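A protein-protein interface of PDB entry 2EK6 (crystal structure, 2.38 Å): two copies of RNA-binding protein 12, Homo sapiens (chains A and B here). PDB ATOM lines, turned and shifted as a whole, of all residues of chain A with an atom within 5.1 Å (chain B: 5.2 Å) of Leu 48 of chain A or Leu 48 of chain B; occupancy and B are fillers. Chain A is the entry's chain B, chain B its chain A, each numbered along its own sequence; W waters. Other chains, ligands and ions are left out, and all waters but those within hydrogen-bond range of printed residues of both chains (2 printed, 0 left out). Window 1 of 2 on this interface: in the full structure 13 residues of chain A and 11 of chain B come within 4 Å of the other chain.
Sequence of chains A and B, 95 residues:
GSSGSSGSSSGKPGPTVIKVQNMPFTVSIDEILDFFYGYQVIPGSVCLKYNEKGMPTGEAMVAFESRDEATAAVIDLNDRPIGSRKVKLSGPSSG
Water W1 bridges the backbone carbonyl oxygen of Tyr 50 of chain A and the backbone NH of Val 46 of chain B.
Water W2 bridges the backbone carbonyl oxygen (O) of Val 46 of chain B and the backbone carbonyl oxygen (O) of Tyr 50 of chain A.
The backbone carbonyl oxygen (O) of Glu 59 of chain B lies within hydrogen-bond range of the backbone NH (N) of Lys 49 of chain B, 3.0 Å away.
N of Lys 49 of chain A lies within hydrogen-bond range of O of Glu 59 of chain A, at 2.9 Å.
Val 46 of chain A touches Leu 48 of chain B, but with the chains exchanged Leu 48 of chain A does not touch Val 46 of chain B (4.1 Å).
Val 46 of chain A touches Lys 49 of chain B, and with the chains exchanged Lys 49 of chain A touches Val 46 of chain B.
Cys 47 of chain A touches Lys 49 of chain B, and with the chains exchanged Lys 49 of chain A touches Cys 47 of chain B.
Leu 48 of chain B touches its own counterpart, Leu 48 of chain A.
Of the 16 pairs that touch across the chains among the printed residues, 15 have their exchanged pair printed and touching as well.
The backbone NH (N) of Leu 48 of chain B lies within hydrogen-bond range of the side-chain sulfur (SG) of Cys 47 of chain A, at 3.2 Å.
The side-chain hydroxyl of Tyr 50 of chain B lies within hydrogen-bond range of the side-chain hydroxyl of Tyr 50 of chain A (3.0 Å).
The backbone carbonyl oxygen (O) of Val 46 of chain B is in hydrogen-bond range of the backbone NH (N) of Tyr 50 of chain A, at 3.0 Å.
N of Leu 48 of chain B is in hydrogen-bond range of O of Leu 48 of chain A, 2.7 Å away.
The backbone carbonyl oxygen (O) of Val 46 of chain A sits at hydrogen-bond distance from the backbone NH (N) of Tyr 50 of chain B (3.1 Å).
The side-chain sulfur (SG) of Cys 47 of chain A lies close to the backbone NH (N) of Lys 49 of chain B, 3.7 Å away.
SG of Cys 47 of chain A is disulfide-bonded to SG of Cys 47 of chain B (2.0 Å).
Printed residues of chain A that touch a printed residue of chain B: Ile 29, Val 46, Cys 47, Leu 48, Lys 49 and Tyr 50.
Hydrophobic or aromatic side chains of chain A that line the printed part of chain B: Ile 29, Leu 48 and Tyr 50.
Of the 10 printed residues of chain B, 6 touch a printed residue of chain A.
Hydrophobic or aromatic side chains of chain B within 4 Å of the printed part of chain A: Ile 29, Leu 48 and Tyr 50.
Among the printed residues, 16 pairs touch across the chains.
Among the printed residues, no Asp or Glu carboxylate lies within 4 Å of a Lys or Arg side-chain nitrogen of the other chain.
Among the printed residues, pairs that only touch across the chains: Leu 48 of chain A with Cys 47 of chain B (3.0 Å), Val 46 of chain A with Lys 49 of chain B (3.3 Å), Tyr 50 of chain A with Leu 48 of chain B (3.6 Å), Ile 29 of chain A with Tyr 50 of chain B (3.6 Å), Lys 49 of chain A with Cys 47 of chain B (3.6 Å), Lys 49 of chain A with Val 46 of chain B (3.6 Å), Tyr 50 of chain A with Ile 29 of chain B (3.8 Å), Val 46 of chain A with Leu 48 of chain B (3.9 Å) and Leu 48 of chain A with Tyr 50 of chain B (3.9 Å).
Printed residues of chain B within 4 Å of Val 46 of chain A: Leu 48, Lys 49 and Tyr 50.
Printed residues of chain B within 4 Å of Cys 47 of chain A: Cys 47 (2.0 Å), Leu 48 (3.2 Å) and Lys 49 (3.6 Å).
Leu 48 of chain A touches three residues of chain B.
Of the printed residues of chain A, Val 46 of chain B touches Lys 49 and Tyr 50.
Leu 48 of chain B touches just these residues of chain A: Val 46, Cys 47, Leu 48 and Tyr 50.
Of the printed residues of chain A, Lys 49 of chain B touches Val 46 (3.3 Å) and Cys 47 (3.6 Å).
The nearest printed residue of chain A that does not touch Lys 49 of chain B is Leu 48 of chain A (4.6 Å).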
ATOM      1  N   MET A  23      17.862 -33.361  15.336  1.00  0.00           N
ATOM      2  CA  MET A  23      17.939 -31.989  14.832  1.00  0.00           C
ATOM      3  C   MET A  23      18.742 -31.210  15.877  1.00  0.00           C
ATOM      4  O   MET A  23      18.715 -31.552  17.061  1.00  0.00           O
ATOM      5  CB  MET A  23      16.551 -31.332  14.749  1.00  0.00           C
ATOM      6  CG  MET A  23      15.459 -32.075  14.008  1.00  0.00           C
ATOM      7  SD  MET A  23      13.973 -31.017  13.782  1.00  0.00           S
ATOM      8  CE  MET A  23      13.343 -30.919  15.430  1.00  0.00           C
ATOM      9  N   VAL A  27      16.555 -25.052  16.450  1.00  0.00           N
ATOM     10  CA  VAL A  27      16.133 -25.130  15.062  1.00  0.00           C
ATOM     11  C   VAL A  27      14.882 -24.252  14.904  1.00  0.00           C
ATOM     12  O   VAL A  27      14.137 -24.049  15.862  1.00  0.00           O
ATOM     13  CB  VAL A  27      15.797 -26.591  14.669  1.00  0.00           C
ATOM     14  CG1 VAL A  27      14.747 -27.141  15.602  1.00  0.00           C
ATOM     15  CG2 VAL A  27      15.298 -26.660  13.227  1.00  0.00           C
ATOM     16  N   ILE A  29      11.264 -23.359  12.586  1.00  0.00           N
ATOM     17  CA  ILE A  29      10.267 -24.049  11.777  1.00  0.00           C
ATOM     18  C   ILE A  29      10.581 -23.739  10.338  1.00  0.00           C
ATOM     19  O   ILE A  29      10.538 -24.608   9.462  1.00  0.00           O
ATOM     20  CB  ILE A  29       8.848 -23.542  12.054  1.00  0.00           C
ATOM     21  CG1 ILE A  29       8.537 -23.670  13.545  1.00  0.00           C
ATOM     22  CG2 ILE A  29       7.853 -24.316  11.206  1.00  0.00           C
ATOM     23  CD1 ILE A  29       8.728 -25.076  14.108  1.00  0.00           C
ATOM     24  N   ILE A  32      12.929 -26.208   9.266  1.00  0.00           N
ATOM     25  CA  ILE A  32      12.349 -27.547   9.143  1.00  0.00           C
ATOM     26  C   ILE A  32      11.532 -27.677   7.856  1.00  0.00           C
ATOM     27  O   ILE A  32      11.641 -28.672   7.134  1.00  0.00           O
ATOM     28  CB  ILE A  32      11.424 -27.868  10.343  1.00  0.00           C
ATOM     29  CG1 ILE A  32      12.237 -27.932  11.633  1.00  0.00           C
ATOM     30  CG2 ILE A  32      10.685 -29.175  10.102  1.00  0.00           C
ATOM     31  CD1 ILE A  32      11.403 -28.156  12.857  1.00  0.00           C
ATOM     32  N   VAL A  46       3.802 -28.929  12.587  1.00  0.00           N
ATOM     33  CA  VAL A  46       5.127 -29.129  13.147  1.00  0.00           C
ATOM     34  C   VAL A  46       5.200 -28.806  14.626  1.00  0.00           C
ATOM     35  O   VAL A  46       5.182 -27.648  15.072  1.00  0.00           O
ATOM     36  CB  VAL A  46       6.208 -28.400  12.376  1.00  0.00           C
ATOM     37  CG1 VAL A  46       7.575 -28.887  12.846  1.00  0.00           C
ATOM     38  CG2 VAL A  46       6.018 -28.715  10.910  1.00  0.00           C
ATOM     39  N   CYS A  47       5.194 -29.920  15.348  1.00  0.00           N
ATOM     40  CA  CYS A  47       5.270 -30.022  16.774  1.00  0.00           C
ATOM     41  C   CYS A  47       6.605 -30.232  17.430  1.00  0.00           C
ATOM     42  O   CYS A  47       7.095 -31.351  17.369  1.00  0.00           O
ATOM     43  CB  CYS A  47       4.473 -31.180  17.187  1.00  0.00           C
ATOM     44  SG  CYS A  47       3.582 -30.770  18.785  1.00  0.00           S
ATOM     45  N   LEU A  48       7.166 -29.231  18.123  1.00  0.00           N
ATOM     46  CA  LEU A  48       8.467 -29.478  18.779  1.00  0.00           C
ATOM     47  C   LEU A  48       8.232 -30.183  20.112  1.00  0.00           C
ATOM     48  O   LEU A  48       7.392 -29.757  20.898  1.00  0.00           O
ATOM     49  CB  LEU A  48       9.267 -28.200  19.041  1.00  0.00           C
ATOM     50  CG  LEU A  48       9.350 -27.132  17.950  1.00  0.00           C
ATOM     51  CD1 LEU A  48      10.408 -26.083  18.308  1.00  0.00           C
ATOM     52  CD2 LEU A  48       9.678 -27.785  16.617  1.00  0.00           C
ATOM     53  N   LYS A  49       8.996 -31.243  20.374  1.00  0.00           N
ATOM     54  CA  LYS A  49       8.846 -32.033  21.597  1.00  0.00           C
ATOM     55  C   LYS A  49       9.681 -31.574  22.783  1.00  0.00           C
ATOM     56  O   LYS A  49      10.766 -31.035  22.615  1.00  0.00           O
ATOM     57  CB  LYS A  49       9.143 -33.503  21.291  1.00  0.00           C
ATOM     58  CG  LYS A  49       8.312 -34.043  20.129  1.00  0.00           C
ATOM     59  CD  LYS A  49       8.373 -35.559  20.054  1.00  0.00           C
ATOM     60  CE  LYS A  49       7.884 -36.171  21.355  1.00  0.00           C
ATOM     61  NZ  LYS A  49       7.680 -37.639  21.289  1.00  0.00           N
ATOM     62  N   TYR A  50       9.158 -31.807  23.986  1.00  0.00           N
ATOM     63  CA  TYR A  50       9.824 -31.426  25.233  1.00  0.00           C
ATOM     64  C   TYR A  50       9.777 -32.597  26.198  1.00  0.00           C
ATOM     65  O   TYR A  50       8.845 -33.398  26.148  1.00  0.00           O
ATOM     66  CB  TYR A  50       9.098 -30.239  25.893  1.00  0.00           C
ATOM     67  CG  TYR A  50       8.993 -29.020  25.015  1.00  0.00           C
ATOM     68  CD1 TYR A  50       8.121 -28.993  23.922  1.00  0.00           C
ATOM     69  CD2 TYR A  50       9.845 -27.933  25.210  1.00  0.00           C
ATOM     70  CE1 TYR A  50       8.113 -27.922  23.042  1.00  0.00           C
ATOM     71  CE2 TYR A  50       9.850 -26.857  24.334  1.00  0.00           C
ATOM     72  CZ  TYR A  50       8.980 -26.857  23.252  1.00  0.00           C
ATOM     73  OH  TYR A  50       8.955 -25.785  22.392  1.00  0.00           O
ATOM     74  N   GLU A  59      13.705 -33.131  18.922  1.00  0.00           N
ATOM     75  CA  GLU A  59      12.712 -33.959  18.249  1.00  0.00           C
ATOM     76  C   GLU A  59      11.418 -33.236  17.929  1.00  0.00           C
ATOM     77  O   GLU A  59      11.035 -32.279  18.596  1.00  0.00           O
ATOM     78  CB  GLU A  59      12.414 -35.181  19.106  1.00  0.00           C
ATOM     79  CG  GLU A  59      13.523 -36.168  19.051  1.00  0.00           C
ATOM     80  CD  GLU A  59      13.380 -37.223  20.077  1.00  0.00           C
ATOM     81  OE1 GLU A  59      12.222 -37.573  20.389  1.00  0.00           O
ATOM     82  OE2 GLU A  59      14.424 -37.706  20.561  1.00  0.00           O
ATOM     83  N   ALA A  60      10.736 -33.714  16.904  1.00  0.00           N
ATOM     84  CA  ALA A  60       9.496 -33.099  16.498  1.00  0.00           C
ATOM     85  C   ALA A  60       8.582 -34.128  15.839  1.00  0.00           C
ATOM     86  O   ALA A  60       8.983 -35.272  15.597  1.00  0.00           O
ATOM     87  CB  ALA A  60       9.794 -31.950  15.537  1.00  0.00           C
ATOM     88  N   MET B  23      -4.690 -22.409  23.049  1.00  0.00           N
ATOM     89  CA  MET B  23      -3.900 -22.146  24.248  1.00  0.00           C
ATOM     90  C   MET B  23      -3.380 -20.711  24.252  1.00  0.00           C
ATOM     91  O   MET B  23      -3.225 -20.094  23.193  1.00  0.00           O
ATOM     92  CB  MET B  23      -2.709 -23.125  24.323  1.00  0.00           C
ATOM     93  CG  MET B  23      -3.066 -24.557  24.737  1.00  0.00           C
ATOM     94  SD  MET B  23      -1.706 -25.773  24.532  1.00  0.00           S
ATOM     95  CE  MET B  23      -0.908 -25.549  25.843  1.00  0.00           C
ATOM     96  N   ILE B  29       5.473 -25.625  29.741  1.00  0.00           N
ATOM     97  CA  ILE B  29       5.266 -27.034  29.762  1.00  0.00           C
ATOM     98  C   ILE B  29       4.667 -27.413  31.138  1.00  0.00           C
ATOM     99  O   ILE B  29       3.727 -28.224  31.229  1.00  0.00           O
ATOM    100  CB  ILE B  29       6.617 -27.729  29.397  1.00  0.00           C
ATOM    101  CG1 ILE B  29       6.881 -27.538  27.883  1.00  0.00           C
ATOM    102  CG2 ILE B  29       6.615 -29.217  29.806  1.00  0.00           C
ATOM    103  CD1 ILE B  29       5.841 -28.166  26.954  1.00  0.00           C
ATOM    104  N   ILE B  32       0.821 -26.837  31.154  1.00  0.00           N
ATOM    105  CA  ILE B  32       0.076 -27.847  30.393  1.00  0.00           C
ATOM    106  C   ILE B  32      -0.098 -29.138  31.189  1.00  0.00           C
ATOM    107  O   ILE B  32      -1.175 -29.734  31.195  1.00  0.00           O
ATOM    108  CB  ILE B  32       0.799 -28.155  29.060  1.00  0.00           C
ATOM    109  CG1 ILE B  32       0.596 -26.988  28.093  1.00  0.00           C
ATOM    110  CG2 ILE B  32       0.291 -29.445  28.456  1.00  0.00           C
ATOM    111  CD1 ILE B  32       1.402 -27.097  26.834  1.00  0.00           C
ATOM    112  N   VAL B  46       4.604 -34.095  25.635  1.00  0.00           N
ATOM    113  CA  VAL B  46       4.124 -32.832  25.078  1.00  0.00           C
ATOM    114  C   VAL B  46       4.984 -32.274  23.978  1.00  0.00           C
ATOM    115  O   VAL B  46       6.201 -32.112  24.096  1.00  0.00           O
ATOM    116  CB  VAL B  46       3.959 -31.753  26.148  1.00  0.00           C
ATOM    117  CG1 VAL B  46       3.511 -30.446  25.500  1.00  0.00           C
ATOM    118  CG2 VAL B  46       2.940 -32.220  27.169  1.00  0.00           C
ATOM    119  N   CYS B  47       4.313 -31.940  22.900  1.00  0.00           N
ATOM    120  CA  CYS B  47       5.012 -31.442  21.749  1.00  0.00           C
ATOM    121  C   CYS B  47       4.172 -30.162  21.330  1.00  0.00           C
ATOM    122  O   CYS B  47       2.935 -30.188  21.208  1.00  0.00           O
ATOM    123  CB  CYS B  47       5.061 -32.609  20.736  1.00  0.00           C
ATOM    124  SG  CYS B  47       3.606 -32.614  19.679  1.00  0.00           S
ATOM    125  N   LEU B  48       4.839 -29.014  21.202  1.00  0.00           N
ATOM    126  CA  LEU B  48       4.157 -27.750  20.886  1.00  0.00           C
ATOM    127  C   LEU B  48       4.255 -27.348  19.428  1.00  0.00           C
ATOM    128  O   LEU B  48       5.354 -27.219  18.904  1.00  0.00           O
ATOM    129  CB  LEU B  48       4.711 -26.603  21.767  1.00  0.00           C
ATOM    130  CG  LEU B  48       4.737 -26.778  23.293  1.00  0.00           C
ATOM    131  CD1 LEU B  48       5.309 -25.528  23.947  1.00  0.00           C
ATOM    132  CD2 LEU B  48       3.340 -27.063  23.825  1.00  0.00           C
ATOM    133  N   LYS B  49       3.109 -27.130  18.787  1.00  0.00           N
ATOM    134  CA  LYS B  49       3.066 -26.758  17.379  1.00  0.00           C
ATOM    135  C   LYS B  49       3.288 -25.267  17.128  1.00  0.00           C
ATOM    136  O   LYS B  49       2.730 -24.411  17.809  1.00  0.00           O
ATOM    137  CB  LYS B  49       1.735 -27.174  16.771  1.00  0.00           C
ATOM    138  CG  LYS B  49       1.397 -28.640  16.933  1.00  0.00           C
ATOM    139  CD  LYS B  49       0.098 -28.965  16.202  1.00  0.00           C
ATOM    140  CE  LYS B  49      -0.199 -30.438  16.260  1.00  0.00           C
ATOM    141  NZ  LYS B  49      -1.516 -30.743  15.654  1.00  0.00           N
ATOM    142  N   TYR B  50       4.109 -24.973  16.129  1.00  0.00           N
ATOM    143  CA  TYR B  50       4.442 -23.603  15.753  1.00  0.00           C
ATOM    144  C   TYR B  50       4.164 -23.434  14.281  1.00  0.00           C
ATOM    145  O   TYR B  50       3.980 -24.415  13.572  1.00  0.00           O
ATOM    146  CB  TYR B  50       5.922 -23.336  15.987  1.00  0.00           C
ATOM    147  CG  TYR B  50       6.338 -23.363  17.430  1.00  0.00           C
ATOM    148  CD1 TYR B  50       6.392 -24.558  18.140  1.00  0.00           C
ATOM    149  CD2 TYR B  50       6.691 -22.188  18.084  1.00  0.00           C
ATOM    150  CE1 TYR B  50       6.792 -24.578  19.466  1.00  0.00           C
ATOM    151  CE2 TYR B  50       7.091 -22.195  19.397  1.00  0.00           C
ATOM    152  CZ  TYR B  50       7.142 -23.388  20.087  1.00  0.00           C
ATOM    153  OH  TYR B  50       7.554 -23.374  21.399  1.00  0.00           O
ATOM    154  N   GLU B  59      -1.538 -24.712  19.745  1.00  0.00           N
ATOM    155  CA  GLU B  59      -1.878 -26.129  19.704  1.00  0.00           C
ATOM    156  C   GLU B  59      -0.705 -26.994  20.150  1.00  0.00           C
ATOM    157  O   GLU B  59       0.445 -26.584  20.080  1.00  0.00           O
ATOM    158  CB  GLU B  59      -2.326 -26.550  18.298  1.00  0.00           C
ATOM    159  CG  GLU B  59      -3.476 -25.716  17.747  1.00  0.00           C
ATOM    160  CD  GLU B  59      -4.139 -26.350  16.536  1.00  0.00           C
ATOM    161  OE1 GLU B  59      -3.440 -27.005  15.743  1.00  0.00           O
ATOM    162  OE2 GLU B  59      -5.363 -26.185  16.369  1.00  0.00           O
ATOM    163  N   ALA B  60      -1.018 -28.194  20.621  1.00  0.00           N
ATOM    164  CA  ALA B  60      -0.012 -29.130  21.091  1.00  0.00           C
ATOM    165  C   ALA B  60      -0.599 -30.535  21.101  1.00  0.00           C
ATOM    166  O   ALA B  60      -1.810 -30.707  20.956  1.00  0.00           O
ATOM    167  CB  ALA B  60       0.452 -28.734  22.507  1.00  0.00           C
HETATM  168  O   HOH W   1       6.693 -33.241  27.514  1.00  0.00           O
HETATM  169  O   HOH W   2       7.485 -34.517  23.889  1.00  0.00           O
